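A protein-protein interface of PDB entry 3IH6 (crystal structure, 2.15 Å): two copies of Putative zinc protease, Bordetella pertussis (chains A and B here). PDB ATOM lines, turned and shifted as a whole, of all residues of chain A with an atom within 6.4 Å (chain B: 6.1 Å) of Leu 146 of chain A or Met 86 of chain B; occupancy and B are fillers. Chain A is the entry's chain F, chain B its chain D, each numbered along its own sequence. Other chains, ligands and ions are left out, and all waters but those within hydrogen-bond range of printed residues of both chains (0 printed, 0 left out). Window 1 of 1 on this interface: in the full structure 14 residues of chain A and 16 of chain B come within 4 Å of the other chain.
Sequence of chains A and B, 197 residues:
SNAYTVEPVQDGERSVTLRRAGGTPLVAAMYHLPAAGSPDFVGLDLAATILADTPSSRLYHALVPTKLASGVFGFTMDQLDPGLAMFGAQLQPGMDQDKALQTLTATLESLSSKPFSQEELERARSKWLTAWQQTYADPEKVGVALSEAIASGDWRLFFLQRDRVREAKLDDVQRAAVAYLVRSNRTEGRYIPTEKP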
ATOM      1  N   LYS A 141      36.125  29.727  21.670  1.00  0.00           N
ATOM      2  CA  LYS A 141      35.355  29.137  20.589  1.00  0.00           C
ATOM      3  C   LYS A 141      34.456  28.019  21.139  1.00  0.00           C
ATOM      4  O   LYS A 141      33.295  27.899  20.714  1.00  0.00           O
ATOM      5  CB  LYS A 141      36.285  28.647  19.480  1.00  0.00           C
ATOM      6  CG  LYS A 141      37.150  29.770  18.893  1.00  0.00           C
ATOM      7  CD  LYS A 141      38.126  29.246  17.822  1.00  0.00           C
ATOM      8  CE  LYS A 141      38.937  30.383  17.260  1.00  0.00           C
ATOM      9  NZ  LYS A 141      39.734  29.962  16.053  1.00  0.00           N
ATOM     10  N   VAL A 142      34.981  27.236  22.090  1.00  0.00           N
ATOM     11  CA  VAL A 142      34.188  26.210  22.801  1.00  0.00           C
ATOM     12  C   VAL A 142      32.936  26.778  23.520  1.00  0.00           C
ATOM     13  O   VAL A 142      31.829  26.193  23.443  1.00  0.00           O
ATOM     14  CB  VAL A 142      35.077  25.409  23.819  1.00  0.00           C
ATOM     15  CG1 VAL A 142      34.239  24.452  24.692  1.00  0.00           C
ATOM     16  CG2 VAL A 142      36.118  24.624  23.090  1.00  0.00           C
ATOM     17  N   GLY A 143      33.111  27.870  24.257  1.00  0.00           N
ATOM     18  CA  GLY A 143      31.981  28.556  24.895  1.00  0.00           C
ATOM     19  C   GLY A 143      30.908  28.967  23.888  1.00  0.00           C
ATOM     20  O   GLY A 143      29.715  28.830  24.152  1.00  0.00           O
ATOM     21  N   VAL A 144      31.336  29.438  22.725  1.00  0.00           N
ATOM     22  CA  VAL A 144      30.408  29.719  21.617  1.00  0.00           C
ATOM     23  C   VAL A 144      29.753  28.438  21.125  1.00  0.00           C
ATOM     24  O   VAL A 144      28.541  28.396  20.971  1.00  0.00           O
ATOM     25  CB  VAL A 144      31.094  30.455  20.439  1.00  0.00           C
ATOM     26  CG1 VAL A 144      30.107  30.700  19.310  1.00  0.00           C
ATOM     27  CG2 VAL A 144      31.664  31.802  20.904  1.00  0.00           C
ATOM     28  N   ALA A 145      30.555  27.383  20.939  1.00  0.00           N
ATOM     29  CA  ALA A 145      30.049  26.130  20.394  1.00  0.00           C
ATOM     30  C   ALA A 145      29.065  25.451  21.356  1.00  0.00           C
ATOM     31  O   ALA A 145      28.042  24.935  20.932  1.00  0.00           O
ATOM     32  CB  ALA A 145      31.205  25.190  19.982  1.00  0.00           C
ATOM     33  N   LEU A 146      29.345  25.516  22.652  1.00  0.00           N
ATOM     34  CA  LEU A 146      28.418  25.015  23.670  1.00  0.00           C
ATOM     35  C   LEU A 146      27.094  25.803  23.706  1.00  0.00           C
ATOM     36  O   LEU A 146      26.030  25.201  23.568  1.00  0.00           O
ATOM     37  CB  LEU A 146      29.064  24.971  25.057  1.00  0.00           C
ATOM     38  CG  LEU A 146      30.089  23.855  25.220  1.00  0.00           C
ATOM     39  CD1 LEU A 146      30.932  24.049  26.504  1.00  0.00           C
ATOM     40  CD2 LEU A 146      29.413  22.481  25.192  1.00  0.00           C
ATOM     41  N   SER A 147      27.149  27.135  23.828  1.00  0.00           N
ATOM     42  CA  SER A 147      25.903  27.900  23.789  1.00  0.00           C
ATOM     43  C   SER A 147      25.090  27.752  22.497  1.00  0.00           C
ATOM     44  O   SER A 147      23.873  27.805  22.555  1.00  0.00           O
ATOM     45  CB  SER A 147      26.058  29.367  24.212  1.00  0.00           C
ATOM     46  OG  SER A 147      26.743  30.115  23.259  1.00  0.00           O
ATOM     47  N   GLU A 148      25.730  27.534  21.353  1.00  0.00           N
ATOM     48  CA  GLU A 148      24.978  27.192  20.118  1.00  0.00           C
ATOM     49  C   GLU A 148      24.274  25.823  20.232  1.00  0.00           C
ATOM     50  O   GLU A 148      23.101  25.669  19.837  1.00  0.00           O
ATOM     51  CB  GLU A 148      25.872  27.223  18.872  1.00  0.00           C
ATOM     52  CG  GLU A 148      26.311  28.622  18.429  1.00  0.00           C
ATOM     53  CD  GLU A 148      27.425  28.591  17.373  1.00  0.00           C
ATOM     54  OE1 GLU A 148      28.198  27.614  17.308  1.00  0.00           O
ATOM     55  OE2 GLU A 148      27.553  29.560  16.609  1.00  0.00           O
ATOM     56  N   ALA A 149      25.002  24.839  20.756  1.00  0.00           N
ATOM     57  CA  ALA A 149      24.432  23.530  21.126  1.00  0.00           C
ATOM     58  C   ALA A 149      23.222  23.624  22.081  1.00  0.00           C
ATOM     59  O   ALA A 149      22.211  22.966  21.841  1.00  0.00           O
ATOM     60  CB  ALA A 149      25.528  22.607  21.721  1.00  0.00           C
ATOM     61  N   ILE A 150      23.329  24.409  23.159  1.00  0.00           N
ATOM     62  CA  ILE A 150      22.168  24.698  24.027  1.00  0.00           C
ATOM     63  C   ILE A 150      21.008  25.363  23.258  1.00  0.00           C
ATOM     64  O   ILE A 150      19.853  24.971  23.428  1.00  0.00           O
ATOM     65  CB  ILE A 150      22.517  25.566  25.267  1.00  0.00           C
ATOM     66  CG1 ILE A 150      23.539  24.855  26.150  1.00  0.00           C
ATOM     67  CG2 ILE A 150      21.220  25.945  26.100  1.00  0.00           C
ATOM     68  CD1 ILE A 150      24.274  25.777  27.121  1.00  0.00           C
ATOM     69  N   ALA A 151      21.323  26.364  22.427  1.00  0.00           N
ATOM     70  CA  ALA A 151      20.341  27.012  21.527  1.00  0.00           C
ATOM     71  C   ALA A 151      19.621  26.014  20.561  1.00  0.00           C
ATOM     72  O   ALA A 151      18.467  26.219  20.200  1.00  0.00           O
ATOM     73  CB  ALA A 151      21.008  28.145  20.739  1.00  0.00           C
ATOM     74  N   ASP A 154      20.295  21.084  23.193  1.00  0.00           N
ATOM     75  CA  ASP A 154      21.073  20.041  23.879  1.00  0.00           C
ATOM     76  C   ASP A 154      22.559  20.361  23.888  1.00  0.00           C
ATOM     77  O   ASP A 154      23.242  20.277  22.851  1.00  0.00           O
ATOM     78  CB  ASP A 154      20.831  18.665  23.235  1.00  0.00           C
ATOM     79  CG  ASP A 154      21.634  17.527  23.907  1.00  0.00           C
ATOM     80  OD1 ASP A 154      22.361  17.724  24.914  1.00  0.00           O
ATOM     81  OD2 ASP A 154      21.532  16.404  23.394  1.00  0.00           O
ATOM     82  N   TRP A 155      23.049  20.716  25.070  1.00  0.00           N
ATOM     83  CA  TRP A 155      24.444  21.082  25.289  1.00  0.00           C
ATOM     84  C   TRP A 155      25.429  19.971  24.876  1.00  0.00           C
ATOM     85  O   TRP A 155      26.571  20.243  24.528  1.00  0.00           O
ATOM     86  CB  TRP A 155      24.646  21.437  26.761  1.00  0.00           C
ATOM     87  CG  TRP A 155      24.520  20.257  27.711  1.00  0.00           C
ATOM     88  CD1 TRP A 155      23.406  19.883  28.426  1.00  0.00           C
ATOM     89  CD2 TRP A 155      25.551  19.339  28.077  1.00  0.00           C
ATOM     90  NE1 TRP A 155      23.684  18.787  29.200  1.00  0.00           N
ATOM     91  CE2 TRP A 155      24.992  18.429  29.000  1.00  0.00           C
ATOM     92  CE3 TRP A 155      26.889  19.177  27.689  1.00  0.00           C
ATOM     93  CZ2 TRP A 155      25.733  17.364  29.547  1.00  0.00           C
ATOM     94  CZ3 TRP A 155      27.614  18.157  28.229  1.00  0.00           C
ATOM     95  CH2 TRP A 155      27.042  17.253  29.156  1.00  0.00           C
ATOM     96  N   ARG A 156      24.975  18.726  24.936  1.00  0.00           N
ATOM     97  CA  ARG A 156      25.792  17.558  24.548  1.00  0.00           C
ATOM     98  C   ARG A 156      26.228  17.565  23.066  1.00  0.00           C
ATOM     99  O   ARG A 156      27.213  16.911  22.693  1.00  0.00           O
ATOM    100  CB  ARG A 156      25.057  16.245  24.880  1.00  0.00           C
ATOM    101  CG  ARG A 156      24.541  16.138  26.338  1.00  0.00           C
ATOM    102  CD  ARG A 156      23.542  15.003  26.586  1.00  0.00           C
ATOM    103  NE  ARG A 156      22.495  14.911  25.561  1.00  0.00           N
ATOM    104  CZ  ARG A 156      22.427  13.954  24.626  1.00  0.00           C
ATOM    105  NH1 ARG A 156      23.332  12.964  24.576  1.00  0.00           N
ATOM    106  NH2 ARG A 156      21.437  13.968  23.747  1.00  0.00           N
ATOM    107  N   PHE A 158      27.665  19.426  20.903  1.00  0.00           N
ATOM    108  CA  PHE A 158      29.005  19.793  20.495  1.00  0.00           C
ATOM    109  C   PHE A 158      29.935  18.582  20.523  1.00  0.00           C
ATOM    110  O   PHE A 158      30.728  18.398  19.599  1.00  0.00           O
ATOM    111  CB  PHE A 158      29.542  20.928  21.368  1.00  0.00           C
ATOM    112  CG  PHE A 158      30.998  21.232  21.146  1.00  0.00           C
ATOM    113  CD1 PHE A 158      31.460  21.619  19.911  1.00  0.00           C
ATOM    114  CD2 PHE A 158      31.902  21.142  22.194  1.00  0.00           C
ATOM    115  CE1 PHE A 158      32.817  21.924  19.715  1.00  0.00           C
ATOM    116  CE2 PHE A 158      33.251  21.437  22.002  1.00  0.00           C
ATOM    117  CZ  PHE A 158      33.697  21.828  20.762  1.00  0.00           C
ATOM    118  N   PHE A 159      29.809  17.734  21.542  1.00  0.00           N
ATOM    119  CA  PHE A 159      30.586  16.510  21.589  1.00  0.00           C
ATOM    120  C   PHE A 159      29.947  15.319  20.871  1.00  0.00           C
ATOM    121  O   PHE A 159      30.650  14.520  20.249  1.00  0.00           O
ATOM    122  CB  PHE A 159      30.932  16.137  23.035  1.00  0.00           C
ATOM    123  CG  PHE A 159      31.948  17.057  23.659  1.00  0.00           C
ATOM    124  CD1 PHE A 159      33.312  16.872  23.425  1.00  0.00           C
ATOM    125  CD2 PHE A 159      31.545  18.108  24.475  1.00  0.00           C
ATOM    126  CE1 PHE A 159      34.265  17.732  23.992  1.00  0.00           C
ATOM    127  CE2 PHE A 159      32.498  18.964  25.059  1.00  0.00           C
ATOM    128  CZ  PHE A 159      33.851  18.774  24.813  1.00  0.00           C
ATOM    129  N   TYR B   4      38.537  26.673  30.169  1.00  0.00           N
ATOM    130  CA  TYR B   4      38.603  25.254  29.828  1.00  0.00           C
ATOM    131  C   TYR B   4      40.048  24.831  30.027  1.00  0.00           C
ATOM    132  O   TYR B   4      40.937  25.255  29.301  1.00  0.00           O
ATOM    133  CB  TYR B   4      38.189  25.033  28.375  1.00  0.00           C
ATOM    134  CG  TYR B   4      37.632  23.673  28.132  1.00  0.00           C
ATOM    135  CD1 TYR B   4      36.364  23.504  27.576  1.00  0.00           C
ATOM    136  CD2 TYR B   4      38.361  22.542  28.478  1.00  0.00           C
ATOM    137  CE1 TYR B   4      35.852  22.223  27.360  1.00  0.00           C
ATOM    138  CE2 TYR B   4      37.866  21.275  28.276  1.00  0.00           C
ATOM    139  CZ  TYR B   4      36.612  21.117  27.716  1.00  0.00           C
ATOM    140  OH  TYR B   4      36.155  19.844  27.521  1.00  0.00           O
ATOM    141  N   VAL B  27      30.135  15.502  32.175  1.00  0.00           N
ATOM    142  CA  VAL B  27      29.031  15.915  33.025  1.00  0.00           C
ATOM    143  C   VAL B  27      29.024  17.470  33.022  1.00  0.00           C
ATOM    144  O   VAL B  27      30.054  18.105  32.692  1.00  0.00           O
ATOM    145  CB  VAL B  27      29.189  15.416  34.464  1.00  0.00           C
ATOM    146  CG1 VAL B  27      29.300  13.864  34.539  1.00  0.00           C
ATOM    147  CG2 VAL B  27      30.389  16.122  35.150  1.00  0.00           C
ATOM    148  N   ALA B  28      27.893  18.049  33.427  1.00  0.00           N
ATOM    149  CA  ALA B  28      27.641  19.486  33.387  1.00  0.00           C
ATOM    150  C   ALA B  28      26.573  19.866  34.393  1.00  0.00           C
ATOM    151  O   ALA B  28      25.675  19.083  34.678  1.00  0.00           O
ATOM    152  CB  ALA B  28      27.188  19.908  31.996  1.00  0.00           C
ATOM    153  N   ALA B  29      26.694  21.073  34.942  1.00  0.00           N
ATOM    154  CA  ALA B  29      25.642  21.690  35.749  1.00  0.00           C
ATOM    155  C   ALA B  29      25.503  23.118  35.265  1.00  0.00           C
ATOM    156  O   ALA B  29      26.504  23.786  35.052  1.00  0.00           O
ATOM    157  CB  ALA B  29      25.989  21.660  37.217  1.00  0.00           C
ATOM    158  N   MET B  30      24.257  23.581  35.103  1.00  0.00           N
ATOM    159  CA  MET B  30      23.986  24.886  34.512  1.00  0.00           C
ATOM    160  C   MET B  30      22.984  25.699  35.335  1.00  0.00           C
ATOM    161  O   MET B  30      22.000  25.172  35.816  1.00  0.00           O
ATOM    162  CB  MET B  30      23.554  24.718  33.048  1.00  0.00           C
ATOM    163  CG  MET B  30      24.550  23.900  32.219  1.00  0.00           C
ATOM    164  SD  MET B  30      23.717  22.951  30.773  1.00  0.00           S
ATOM    165  CE  MET B  30      22.837  21.514  31.818  1.00  0.00           C
ATOM    166  N   TYR B  31      23.279  26.981  35.501  1.00  0.00           N
ATOM    167  CA  TYR B  31      22.607  27.852  36.443  1.00  0.00           C
ATOM    168  C   TYR B  31      22.135  29.113  35.751  1.00  0.00           C
ATOM    169  O   TYR B  31      22.884  29.698  34.987  1.00  0.00           O
ATOM    170  CB  TYR B  31      23.605  28.258  37.530  1.00  0.00           C
ATOM    171  CG  TYR B  31      24.169  27.066  38.274  1.00  0.00           C
ATOM    172  CD1 TYR B  31      23.715  26.745  39.541  1.00  0.00           C
ATOM    173  CD2 TYR B  31      25.139  26.253  37.699  1.00  0.00           C
ATOM    174  CE1 TYR B  31      24.212  25.637  40.235  1.00  0.00           C
ATOM    175  CE2 TYR B  31      25.658  25.153  38.384  1.00  0.00           C
ATOM    176  CZ  TYR B  31      25.191  24.852  39.653  1.00  0.00           C
ATOM    177  OH  TYR B  31      25.684  23.739  40.321  1.00  0.00           O
ATOM    178  N   PHE B  73      35.608  22.893  32.866  1.00  0.00           N
ATOM    179  CA  PHE B  73      35.293  24.136  32.188  1.00  0.00           C
ATOM    180  C   PHE B  73      34.190  24.935  32.906  1.00  0.00           C
ATOM    181  O   PHE B  73      33.496  24.412  33.796  1.00  0.00           O
ATOM    182  CB  PHE B  73      34.893  23.876  30.748  1.00  0.00           C
ATOM    183  CG  PHE B  73      33.751  22.907  30.576  1.00  0.00           C
ATOM    184  CD1 PHE B  73      34.004  21.562  30.323  1.00  0.00           C
ATOM    185  CD2 PHE B  73      32.433  23.359  30.621  1.00  0.00           C
ATOM    186  CE1 PHE B  73      32.952  20.670  30.117  1.00  0.00           C
ATOM    187  CE2 PHE B  73      31.370  22.493  30.424  1.00  0.00           C
ATOM    188  CZ  PHE B  73      31.627  21.134  30.158  1.00  0.00           C
ATOM    189  N   GLY B  74      34.056  26.201  32.514  1.00  0.00           N
ATOM    190  CA  GLY B  74      33.015  27.082  33.008  1.00  0.00           C
ATOM    191  C   GLY B  74      32.905  28.339  32.159  1.00  0.00           C
ATOM    192  O   GLY B  74      33.921  28.969  31.832  1.00  0.00           O
ATOM    193  N   PHE B  75      31.664  28.682  31.796  1.00  0.00           N
ATOM    194  CA  PHE B  75      31.367  29.794  30.930  1.00  0.00           C
ATOM    195  C   PHE B  75      30.135  30.540  31.446  1.00  0.00           C
ATOM    196  O   PHE B  75      29.174  29.927  31.898  1.00  0.00           O
ATOM    197  CB  PHE B  75      31.036  29.325  29.495  1.00  0.00           C
ATOM    198  CG  PHE B  75      32.047  28.415  28.888  1.00  0.00           C
ATOM    199  CD1 PHE B  75      31.970  27.025  29.087  1.00  0.00           C
ATOM    200  CD2 PHE B  75      33.060  28.916  28.085  1.00  0.00           C
ATOM    201  CE1 PHE B  75      32.909  26.175  28.521  1.00  0.00           C
ATOM    202  CE2 PHE B  75      33.971  28.068  27.494  1.00  0.00           C
ATOM    203  CZ  PHE B  75      33.906  26.686  27.718  1.00  0.00           C
ATOM    204  N   THR B  76      30.125  31.855  31.311  1.00  0.00           N
ATOM    205  CA  THR B  76      28.850  32.571  31.383  1.00  0.00           C
ATOM    206  C   THR B  76      28.376  32.797  29.956  1.00  0.00           C
ATOM    207  O   THR B  76      29.133  33.275  29.129  1.00  0.00           O
ATOM    208  CB  THR B  76      28.985  33.858  32.172  1.00  0.00           C
ATOM    209  OG1 THR B  76      30.094  34.591  31.657  1.00  0.00           O
ATOM    210  CG2 THR B  76      29.263  33.531  33.641  1.00  0.00           C
ATOM    211  N   MET B  77      27.153  32.375  29.647  1.00  0.00           N
ATOM    212  CA  MET B  77      26.589  32.496  28.299  1.00  0.00           C
ATOM    213  C   MET B  77      25.408  33.479  28.284  1.00  0.00           C
ATOM    214  O   MET B  77      24.263  33.108  28.509  1.00  0.00           O
ATOM    215  CB  MET B  77      26.211  31.109  27.731  1.00  0.00           C
ATOM    216  CG  MET B  77      27.432  30.174  27.598  1.00  0.00           C
ATOM    217  SD  MET B  77      27.050  28.270  27.542  1.00  0.00           S
ATOM    218  CE  MET B  77      28.845  27.599  27.324  1.00  0.00           C
ATOM    219  N   LEU B  84      22.930  31.613  30.962  1.00  0.00           N
ATOM    220  CA  LEU B  84      23.376  30.496  31.808  1.00  0.00           C
ATOM    221  C   LEU B  84      24.807  30.626  32.260  1.00  0.00           C
ATOM    222  O   LEU B  84      25.636  31.210  31.566  1.00  0.00           O
ATOM    223  CB  LEU B  84      23.269  29.146  31.071  1.00  0.00           C
ATOM    224  CG  LEU B  84      21.985  28.636  30.416  1.00  0.00           C
ATOM    225  CD1 LEU B  84      22.283  27.217  29.908  1.00  0.00           C
ATOM    226  CD2 LEU B  84      20.793  28.587  31.359  1.00  0.00           C
ATOM    227  N   ALA B  85      25.084  30.078  33.437  1.00  0.00           N
ATOM    228  CA  ALA B  85      26.423  29.741  33.841  1.00  0.00           C
ATOM    229  C   ALA B  85      26.531  28.232  33.608  1.00  0.00           C
ATOM    230  O   ALA B  85      25.706  27.452  34.104  1.00  0.00           O
ATOM    231  CB  ALA B  85      26.643  30.083  35.313  1.00  0.00           C
ATOM    232  N   MET B  86      27.546  27.813  32.858  1.00  0.00           N
ATOM    233  CA  MET B  86      27.727  26.396  32.604  1.00  0.00           C
ATOM    234  C   MET B  86      29.081  25.879  33.062  1.00  0.00           C
ATOM    235  O   MET B  86      30.128  26.318  32.599  1.00  0.00           O
ATOM    236  CB  MET B  86      27.489  26.039  31.130  1.00  0.00           C
ATOM    237  CG  MET B  86      27.978  24.619  30.798  1.00  0.00           C
ATOM    238  SD  MET B  86      27.804  24.167  28.926  1.00  0.00           S
ATOM    239  CE  MET B  86      27.652  22.238  29.059  1.00  0.00           C
ATOM    240  N   PHE B  87      29.023  24.905  33.950  1.00  0.00           N
ATOM    241  CA  PHE B  87      30.202  24.252  34.515  1.00  0.00           C
ATOM    242  C   PHE B  87      30.156  22.789  34.139  1.00  0.00           C
ATOM    243  O   PHE B  87      29.089  22.235  33.944  1.00  0.00           O
ATOM    244  CB  PHE B  87      30.194  24.424  36.029  1.00  0.00           C
ATOM    245  CG  PHE B  87      30.288  25.853  36.464  1.00  0.00           C
ATOM    246  CD1 PHE B  87      31.537  26.515  36.486  1.00  0.00           C
ATOM    247  CD2 PHE B  87      29.144  26.556  36.825  1.00  0.00           C
ATOM    248  CE1 PHE B  87      31.640  27.826  36.867  1.00  0.00           C
ATOM    249  CE2 PHE B  87      29.227  27.871  37.228  1.00  0.00           C
ATOM    250  CZ  PHE B  87      30.482  28.528  37.245  1.00  0.00           C
ATOM    251  N   GLY B  88      31.299  22.140  34.037  1.00  0.00           N
ATOM    252  CA  GLY B  88      31.307  20.782  33.565  1.00  0.00           C
ATOM    253  C   GLY B  88      32.668  20.155  33.653  1.00  0.00           C
ATOM    254  O   GLY B  88      33.678  20.827  33.952  1.00  0.00           O
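Leu 146 of chain A touches just these residues of chain B: Phe 75 (3.5 Å), Met 77 (3.5 Å) and Met 86 (3.96 Å).
Printed residues of chain A within 4 Å of Met 86 of chain B: Leu 146 and Trp 155.
Of the printed residues of chain A, Met 77 of chain B touches Gly 143 (3.5 Å), Leu 146 (3.5 Å), Ser 147 (3.6 Å) and Ile 150 (3.8 Å).
Printed residues of chain B within 4 Å of Trp 155 of chain A: Ala 28 (3.8 Å), Met 30 (3.8 Å) and Met 86 (3.4 Å).
Printed residues of chain A within 4 Å of Met 30 of chain B: Trp 155.
Of the printed residues of chain B, Ser 147 of chain A touches Met 77.
Gly 88 of chain B touches none of the printed residues of chain A.
The nearest residue of chain B that does not touch Leu 146 of chain A is Phe 73 of chain B (4.2 Å).
Among the printed residues, merely in contact across the chains: Gly 143 of chain A with Phe 75 of chain B, Trp 155 of chain A with Met 86 of chain B, Leu 146 of chain A with Met 77 of chain B, Gly 143 of chain A with Met 77 of chain B, Leu 146 of chain A with Phe 75 of chain B, Ser 147 of chain A with Met 77 of chain B, Val 142 of chain A with Tyr 4 of chain B, Phe 159 of chain A with Tyr 4 of chain B, Ile 150 of chain A with Leu 84 of chain B, Ile 150 of chain A with Met 77 of chain B, Val 142 of chain A with Phe 75 of chain B, Trp 155 of chain A with Met 30 of chain B, Trp 155 of chain A with Ala 28 of chain B and Leu 146 of chain A with Met 86 of chain B.
Of the 16 printed residues of chain A, 7 touch a printed residue of chain B.
Hydrophobic or aromatic side chains of chain A that line the printed part of chain B: Val 142, Leu 146, Ile 150, Trp 155 and Phe 159.
Hydrophobic or aromatic side chains of chain B that line the printed part of chain A: Tyr 4, Ala 28, Met 30, Phe 75, Met 77, Leu 84 and Met 86.
Among the printed residues, no Asp or Glu carboxylate lies within 4 Å of a Lys or Arg side-chain nitrogen of the other chain.
No position is printed for both chains.
Of the 14 pairs that touch across the chains among the printed residues, none has its exchanged pair printed and touching as well.
The backbone NH (N) of Met 77 of chain B is in hydrogen-bond range of the backbone carbonyl oxygen (O) of Leu 84 of chain B.
The backbone carbonyl oxygen (O) of Val 144 of chain A is in hydrogen-bond range of the side-chain hydroxyl (OG) of Ser 147 of chain A (3.4 Å).
The side-chain hydroxyl (OG) of Ser 147 of chain A is in hydrogen-bond range of the backbone carbonyl oxygen (O) of Gly 143 of chain A.
N of Met 86 of chain B is in hydrogen-bond range of O of Phe 75 of chain B (2.8 Å).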
